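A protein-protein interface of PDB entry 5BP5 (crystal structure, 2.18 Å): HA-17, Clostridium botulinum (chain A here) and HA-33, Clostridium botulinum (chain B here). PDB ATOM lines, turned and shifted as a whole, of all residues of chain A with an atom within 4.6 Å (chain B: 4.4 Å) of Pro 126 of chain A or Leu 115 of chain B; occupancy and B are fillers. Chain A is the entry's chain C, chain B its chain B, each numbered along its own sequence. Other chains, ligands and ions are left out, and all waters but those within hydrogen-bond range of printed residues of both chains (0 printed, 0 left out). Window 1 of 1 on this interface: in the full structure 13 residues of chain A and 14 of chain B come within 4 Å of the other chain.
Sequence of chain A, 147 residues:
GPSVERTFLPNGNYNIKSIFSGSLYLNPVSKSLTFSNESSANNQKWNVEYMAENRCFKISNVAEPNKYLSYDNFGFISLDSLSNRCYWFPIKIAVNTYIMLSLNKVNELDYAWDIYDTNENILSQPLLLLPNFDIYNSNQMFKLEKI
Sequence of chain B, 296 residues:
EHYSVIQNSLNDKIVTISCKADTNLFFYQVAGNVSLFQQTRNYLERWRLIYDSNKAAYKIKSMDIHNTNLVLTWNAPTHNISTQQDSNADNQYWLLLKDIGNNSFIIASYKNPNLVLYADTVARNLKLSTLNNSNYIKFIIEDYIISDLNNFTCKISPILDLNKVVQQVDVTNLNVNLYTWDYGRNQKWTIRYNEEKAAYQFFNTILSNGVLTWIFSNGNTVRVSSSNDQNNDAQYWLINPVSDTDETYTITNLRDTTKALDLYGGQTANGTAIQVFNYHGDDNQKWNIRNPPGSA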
ATOM      1  N   SER A  32     -24.061  21.412  36.538  1.00  0.00           N
ATOM      2  CA  SER A  32     -23.504  20.749  35.373  1.00  0.00           C
ATOM      3  C   SER A  32     -22.662  19.552  35.745  1.00  0.00           C
ATOM      4  O   SER A  32     -22.327  19.356  36.900  1.00  0.00           O
ATOM      5  CB  SER A  32     -22.645  21.711  34.574  1.00  0.00           C
ATOM      6  OG  SER A  32     -23.406  22.807  34.124  1.00  0.00           O
ATOM      7  N   LEU A  33     -22.336  18.750  34.737  1.00  0.00           N
ATOM      8  CA  LEU A  33     -21.331  17.693  34.853  1.00  0.00           C
ATOM      9  C   LEU A  33     -20.127  18.074  34.007  1.00  0.00           C
ATOM     10  O   LEU A  33     -20.283  18.600  32.910  1.00  0.00           O
ATOM     11  CB  LEU A  33     -21.875  16.350  34.370  1.00  0.00           C
ATOM     12  CG  LEU A  33     -22.740  15.540  35.320  1.00  0.00           C
ATOM     13  CD1 LEU A  33     -21.992  15.272  36.617  1.00  0.00           C
ATOM     14  CD2 LEU A  33     -24.086  16.219  35.574  1.00  0.00           C
ATOM     15  N   THR A  34     -18.934  17.797  34.527  1.00  0.00           N
ATOM     16  CA  THR A  34     -17.698  18.157  33.851  1.00  0.00           C
ATOM     17  C   THR A  34     -16.567  17.214  34.256  1.00  0.00           C
ATOM     18  O   THR A  34     -16.688  16.457  35.226  1.00  0.00           O
ATOM     19  CB  THR A  34     -17.315  19.636  34.107  1.00  0.00           C
ATOM     20  OG1 THR A  34     -16.442  20.106  33.065  1.00  0.00           O
ATOM     21  CG2 THR A  34     -16.655  19.818  35.480  1.00  0.00           C
ATOM     22  N   PHE A  76     -28.279  19.588  28.530  1.00  0.00           N
ATOM     23  CA  PHE A  76     -27.240  19.215  29.471  1.00  0.00           C
ATOM     24  C   PHE A  76     -27.526  17.890  30.180  1.00  0.00           C
ATOM     25  O   PHE A  76     -28.661  17.628  30.581  1.00  0.00           O
ATOM     26  CB  PHE A  76     -27.107  20.252  30.584  1.00  0.00           C
ATOM     27  CG  PHE A  76     -26.493  21.562  30.180  1.00  0.00           C
ATOM     28  CD1 PHE A  76     -27.193  22.467  29.396  1.00  0.00           C
ATOM     29  CD2 PHE A  76     -25.261  21.946  30.684  1.00  0.00           C
ATOM     30  CE1 PHE A  76     -26.644  23.697  29.070  1.00  0.00           C
ATOM     31  CE2 PHE A  76     -24.713  23.176  30.360  1.00  0.00           C
ATOM     32  CZ  PHE A  76     -25.408  24.054  29.552  1.00  0.00           C
ATOM     33  N   ASP A 114     -22.124  13.647  25.248  1.00  0.00           N
ATOM     34  CA  ASP A 114     -21.295  14.327  24.270  1.00  0.00           C
ATOM     35  C   ASP A 114     -20.519  15.428  24.969  1.00  0.00           C
ATOM     36  O   ASP A 114     -21.089  16.266  25.627  1.00  0.00           O
ATOM     37  CB  ASP A 114     -22.159  14.901  23.148  1.00  0.00           C
ATOM     38  CG  ASP A 114     -21.354  15.322  21.920  1.00  0.00           C
ATOM     39  OD1 ASP A 114     -20.359  16.083  22.041  1.00  0.00           O
ATOM     40  OD2 ASP A 114     -21.775  14.927  20.821  1.00  0.00           O
ATOM     41  N   ILE A 115     -19.211  15.405  24.815  1.00  0.00           N
ATOM     42  CA  ILE A 115     -18.330  16.399  25.423  1.00  0.00           C
ATOM     43  C   ILE A 115     -17.570  17.097  24.303  1.00  0.00           C
ATOM     44  O   ILE A 115     -16.877  16.450  23.540  1.00  0.00           O
ATOM     45  CB  ILE A 115     -17.344  15.729  26.431  1.00  0.00           C
ATOM     46  CG1 ILE A 115     -16.590  16.779  27.258  1.00  0.00           C
ATOM     47  CG2 ILE A 115     -16.398  14.749  25.748  1.00  0.00           C
ATOM     48  CD1 ILE A 115     -17.463  17.479  28.275  1.00  0.00           C
ATOM     49  N   SER A 124     -13.371  22.532  31.432  1.00  0.00           N
ATOM     50  CA  SER A 124     -14.500  23.422  31.697  1.00  0.00           C
ATOM     51  C   SER A 124     -15.730  23.171  30.827  1.00  0.00           C
ATOM     52  O   SER A 124     -16.685  23.941  30.909  1.00  0.00           O
ATOM     53  CB  SER A 124     -14.096  24.895  31.584  1.00  0.00           C
ATOM     54  OG  SER A 124     -13.005  25.184  32.419  1.00  0.00           O
ATOM     55  N   GLN A 125     -15.707  22.120  29.998  1.00  0.00           N
ATOM     56  CA  GLN A 125     -16.834  21.781  29.149  1.00  0.00           C
ATOM     57  C   GLN A 125     -17.884  20.991  29.926  1.00  0.00           C
ATOM     58  O   GLN A 125     -17.554  20.055  30.647  1.00  0.00           O
ATOM     59  CB  GLN A 125     -16.395  20.985  27.916  1.00  0.00           C
ATOM     60  CG  GLN A 125     -15.554  21.779  26.925  1.00  0.00           C
ATOM     61  CD  GLN A 125     -16.331  22.768  26.078  1.00  0.00           C
ATOM     62  OE1 GLN A 125     -17.562  22.828  26.109  1.00  0.00           O
ATOM     63  NE2 GLN A 125     -15.603  23.564  25.315  1.00  0.00           N
ATOM     64  N   PRO A 126     -19.156  21.373  29.785  1.00  0.00           N
ATOM     65  CA  PRO A 126     -20.223  20.574  30.367  1.00  0.00           C
ATOM     66  C   PRO A 126     -20.534  19.374  29.491  1.00  0.00           C
ATOM     67  O   PRO A 126     -20.417  19.452  28.277  1.00  0.00           O
ATOM     68  CB  PRO A 126     -21.405  21.538  30.377  1.00  0.00           C
ATOM     69  CG  PRO A 126     -21.191  22.369  29.162  1.00  0.00           C
ATOM     70  CD  PRO A 126     -19.696  22.516  29.020  1.00  0.00           C
ATOM     71  N   LEU A 127     -20.904  18.267  30.114  1.00  0.00           N
ATOM     72  CA  LEU A 127     -21.319  17.103  29.375  1.00  0.00           C
ATOM     73  C   LEU A 127     -22.723  17.351  28.843  1.00  0.00           C
ATOM     74  O   LEU A 127     -23.628  17.703  29.606  1.00  0.00           O
ATOM     75  CB  LEU A 127     -21.311  15.866  30.264  1.00  0.00           C
ATOM     76  CG  LEU A 127     -21.541  14.529  29.556  1.00  0.00           C
ATOM     77  CD1 LEU A 127     -20.423  14.221  28.571  1.00  0.00           C
ATOM     78  CD2 LEU A 127     -21.662  13.414  30.585  1.00  0.00           C
ATOM     79  N   LEU A 128     -22.889  17.166  27.538  1.00  0.00           N
ATOM     80  CA  LEU A 128     -24.167  17.432  26.887  1.00  0.00           C
ATOM     81  C   LEU A 128     -24.825  16.131  26.417  1.00  0.00           C
ATOM     82  O   LEU A 128     -24.199  15.044  26.460  1.00  0.00           O
ATOM     83  CB  LEU A 128     -23.959  18.408  25.731  1.00  0.00           C
ATOM     84  CG  LEU A 128     -23.357  19.756  26.120  1.00  0.00           C
ATOM     85  CD1 LEU A 128     -23.234  20.637  24.890  1.00  0.00           C
ATOM     86  CD2 LEU A 128     -24.192  20.458  27.189  1.00  0.00           C
ATOM     87  N   TRP B  74     -19.554  33.285  29.758  1.00  0.00           N
ATOM     88  CA  TRP B  74     -20.157  32.026  30.159  1.00  0.00           C
ATOM     89  C   TRP B  74     -19.265  31.356  31.184  1.00  0.00           C
ATOM     90  O   TRP B  74     -18.118  31.019  30.894  1.00  0.00           O
ATOM     91  CB  TRP B  74     -20.399  31.112  28.963  1.00  0.00           C
ATOM     92  CG  TRP B  74     -20.717  29.704  29.346  1.00  0.00           C
ATOM     93  CD1 TRP B  74     -21.421  29.300  30.421  1.00  0.00           C
ATOM     94  CD2 TRP B  74     -20.331  28.517  28.649  1.00  0.00           C
ATOM     95  NE1 TRP B  74     -21.499  27.932  30.458  1.00  0.00           N
ATOM     96  CE2 TRP B  74     -20.833  27.427  29.376  1.00  0.00           C
ATOM     97  CE3 TRP B  74     -19.598  28.270  27.489  1.00  0.00           C
ATOM     98  CZ2 TRP B  74     -20.630  26.109  28.980  1.00  0.00           C
ATOM     99  CZ3 TRP B  74     -19.408  26.969  27.097  1.00  0.00           C
ATOM    100  CH2 TRP B  74     -19.915  25.899  27.845  1.00  0.00           C
ATOM    101  N   PRO B  77     -18.191  25.321  33.433  1.00  0.00           N
ATOM    102  CA  PRO B  77     -19.221  24.518  32.783  1.00  0.00           C
ATOM    103  C   PRO B  77     -20.639  24.773  33.261  1.00  0.00           C
ATOM    104  O   PRO B  77     -21.533  24.050  32.846  1.00  0.00           O
ATOM    105  CB  PRO B  77     -18.829  23.101  33.161  1.00  0.00           C
ATOM    106  CG  PRO B  77     -18.241  23.254  34.524  1.00  0.00           C
ATOM    107  CD  PRO B  77     -17.647  24.632  34.616  1.00  0.00           C
ATOM    108  N   ALA B 108     -24.530  32.183  20.115  1.00  0.00           N
ATOM    109  CA  ALA B 108     -23.899  30.917  20.455  1.00  0.00           C
ATOM    110  C   ALA B 108     -22.510  31.153  21.071  1.00  0.00           C
ATOM    111  O   ALA B 108     -21.775  32.028  20.616  1.00  0.00           O
ATOM    112  CB  ALA B 108     -23.762  30.065  19.197  1.00  0.00           C
ATOM    113  N   SER B 109     -22.164  30.371  22.094  1.00  0.00           N
ATOM    114  CA  SER B 109     -20.843  30.447  22.713  1.00  0.00           C
ATOM    115  C   SER B 109     -19.778  30.007  21.726  1.00  0.00           C
ATOM    116  O   SER B 109     -19.882  28.947  21.125  1.00  0.00           O
ATOM    117  CB  SER B 109     -20.728  29.560  23.953  1.00  0.00           C
ATOM    118  OG  SER B 109     -19.393  29.611  24.469  1.00  0.00           O
ATOM    119  N   ASN B 112     -18.357  26.730  23.093  1.00  0.00           N
ATOM    120  CA  ASN B 112     -19.105  25.558  22.719  1.00  0.00           C
ATOM    121  C   ASN B 112     -20.319  25.964  21.903  1.00  0.00           C
ATOM    122  O   ASN B 112     -21.394  26.234  22.456  1.00  0.00           O
ATOM    123  CB  ASN B 112     -19.467  24.732  23.939  1.00  0.00           C
ATOM    124  CG  ASN B 112     -20.080  23.393  23.573  1.00  0.00           C
ATOM    125  OD1 ASN B 112     -20.647  23.214  22.488  1.00  0.00           O
ATOM    126  ND2 ASN B 112     -19.974  22.440  24.487  1.00  0.00           N
ATOM    127  N   PRO B 113     -20.149  26.004  20.573  1.00  0.00           N
ATOM    128  CA  PRO B 113     -21.171  26.489  19.650  1.00  0.00           C
ATOM    129  C   PRO B 113     -22.467  25.706  19.658  1.00  0.00           C
ATOM    130  O   PRO B 113     -23.371  26.095  18.968  1.00  0.00           O
ATOM    131  CB  PRO B 113     -20.516  26.369  18.273  1.00  0.00           C
ATOM    132  CG  PRO B 113     -19.069  26.231  18.524  1.00  0.00           C
ATOM    133  CD  PRO B 113     -18.895  25.660  19.887  1.00  0.00           C
ATOM    134  N   ASN B 114     -22.511  24.573  20.348  1.00  0.00           N
ATOM    135  CA  ASN B 114     -23.727  23.820  20.541  1.00  0.00           C
ATOM    136  C   ASN B 114     -24.630  24.497  21.560  1.00  0.00           C
ATOM    137  O   ASN B 114     -25.779  24.119  21.680  1.00  0.00           O
ATOM    138  CB  ASN B 114     -23.441  22.402  21.026  1.00  0.00           C
ATOM    139  CG  ASN B 114     -22.686  21.571  20.012  1.00  0.00           C
ATOM    140  OD1 ASN B 114     -23.231  21.179  18.998  1.00  0.00           O
ATOM    141  ND2 ASN B 114     -21.405  21.293  20.295  1.00  0.00           N
ATOM    142  N   LEU B 115     -24.085  25.469  22.307  1.00  0.00           N
ATOM    143  CA  LEU B 115     -24.806  26.129  23.359  1.00  0.00           C
ATOM    144  C   LEU B 115     -25.020  27.574  22.998  1.00  0.00           C
ATOM    145  O   LEU B 115     -24.094  28.251  22.569  1.00  0.00           O
ATOM    146  CB  LEU B 115     -24.058  26.015  24.696  1.00  0.00           C
ATOM    147  CG  LEU B 115     -23.890  24.588  25.197  1.00  0.00           C
ATOM    148  CD1 LEU B 115     -22.990  24.540  26.426  1.00  0.00           C
ATOM    149  CD2 LEU B 115     -25.220  23.948  25.495  1.00  0.00           C
ATOM    150  N   VAL B 116     -26.265  28.026  23.177  1.00  0.00           N
ATOM    151  CA  VAL B 116     -26.665  29.388  22.872  1.00  0.00           C
ATOM    152  C   VAL B 116     -27.403  30.013  24.056  1.00  0.00           C
ATOM    153  O   VAL B 116     -27.901  29.315  24.938  1.00  0.00           O
ATOM    154  CB  VAL B 116     -27.545  29.441  21.609  1.00  0.00           C
ATOM    155  CG1 VAL B 116     -26.919  28.601  20.517  1.00  0.00           C
ATOM    156  CG2 VAL B 116     -28.963  28.935  21.887  1.00  0.00           C
ATOM    157  N   LEU B 128     -28.212  28.808  29.254  1.00  0.00           N
ATOM    158  CA  LEU B 128     -27.793  28.255  27.984  1.00  0.00           C
ATOM    159  C   LEU B 128     -28.691  27.128  27.545  1.00  0.00           C
ATOM    160  O   LEU B 128     -29.351  26.473  28.339  1.00  0.00           O
ATOM    161  CB  LEU B 128     -26.346  27.745  28.075  1.00  0.00           C
ATOM    162  CG  LEU B 128     -25.267  28.815  28.212  1.00  0.00           C
ATOM    163  CD1 LEU B 128     -23.916  28.178  28.455  1.00  0.00           C
ATOM    164  CD2 LEU B 128     -25.203  29.671  26.964  1.00  0.00           C
ATOM    165  N   SER B 129     -28.704  26.892  26.249  1.00  0.00           N
ATOM    166  CA  SER B 129     -29.420  25.755  25.724  1.00  0.00           C
ATOM    167  C   SER B 129     -28.834  25.327  24.414  1.00  0.00           C
ATOM    168  O   SER B 129     -28.246  26.114  23.700  1.00  0.00           O
ATOM    169  CB  SER B 129     -30.904  26.108  25.517  1.00  0.00           C
ATOM    170  OG  SER B 129     -31.552  25.109  24.733  1.00  0.00           O
ATOM    171  N   THR B 130     -29.028  24.063  24.086  1.00  0.00           N
ATOM    172  CA  THR B 130     -28.806  23.613  22.717  1.00  0.00           C
ATOM    173  C   THR B 130     -29.866  24.237  21.827  1.00  0.00           C
ATOM    174  O   THR B 130     -30.902  24.733  22.319  1.00  0.00           O
ATOM    175  CB  THR B 130     -28.819  22.091  22.618  1.00  0.00           C
ATOM    176  OG1 THR B 130     -30.027  21.569  23.158  1.00  0.00           O
ATOM    177  CG2 THR B 130     -27.638  21.524  23.421  1.00  0.00           C
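The backbone carbonyl oxygen of Pro 77 of chain B sits at hydrogen-bond distance from the side-chain hydroxyl of Ser 32 of chain A. The side-chain amide oxygen (OE1) of Gln 125 of chain A is in hydrogen-bond range of the side-chain amide nitrogen (ND2) of Asn 112 of chain B, at 2.9 Å. O of Ser 124 of chain A lies close to N of Pro 77 of chain B (3.2 Å).
Of the printed residues of chain B, Thr 34 of chain A touches Pro 77 (3.8 Å). Of the printed residues of chain B, Phe 76 of chain A touches Leu 115 and Leu 128. Of chain B, only Trp 74 (3.6 Å), Pro 77 (3.5 Å) and Leu 115 (3.9 Å) come within 4 Å of Pro 126 of chain A. The nearest printed residue of chain B that does not touch Pro 126 of chain A is Asn 112 of chain B (4.5 Å). The nearest printed residue of chain A that does not touch Leu 115 of chain B is Gln 125 of chain A (5.7 Å).
Among the printed residues, merely in contact across the chains: Thr 34 of chain A with Pro 77 of chain B (3.8 Å), Phe 76 of chain A with Leu 115 of chain B (3.9 Å), Phe 76 of chain A with Leu 128 of chain B (3.9 Å), Gln 125 of chain A with Pro 77 of chain B (3.98 Å), Pro 126 of chain A with Trp 74 of chain B (3.6 Å), Pro 126 of chain A with Pro 77 of chain B (3.5 Å), Pro 126 of chain A with Leu 115 of chain B (3.9 Å), Leu 128 of chain A with Asn 112 of chain B (3.7 Å) and Leu 128 of chain A with Leu 115 of chain B (3.9 Å).
The side-chain hydroxyl (OG) of Ser 109 of chain B lies within hydrogen-bond range of the backbone NH (N) of Asn 112 of chain B. The backbone carbonyl oxygen (O) of Leu 115 of chain B lies within hydrogen-bond range of the backbone NH (N) of Ser 109 of chain B (2.9 Å). OD1 of Asn 112 of chain B is in hydrogen-bond range of ND2 of Asn 114 of chain B (3.0 Å). The backbone carbonyl oxygen of Gln 125 of chain A is in hydrogen-bond range of the side-chain hydroxyl of Thr 34 of chain A, at 2.7 Å. The backbone carbonyl oxygen (O) of Asp 114 of chain A is in hydrogen-bond range of the backbone NH (N) of Leu 128 of chain A (2.8 Å).
Hydrophobic or aromatic side chains of chain A that line the printed part of chain B: Phe 76, Pro 126 and Leu 128. Of the 12 printed residues of chain B, 5 touch a printed residue of chain A.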
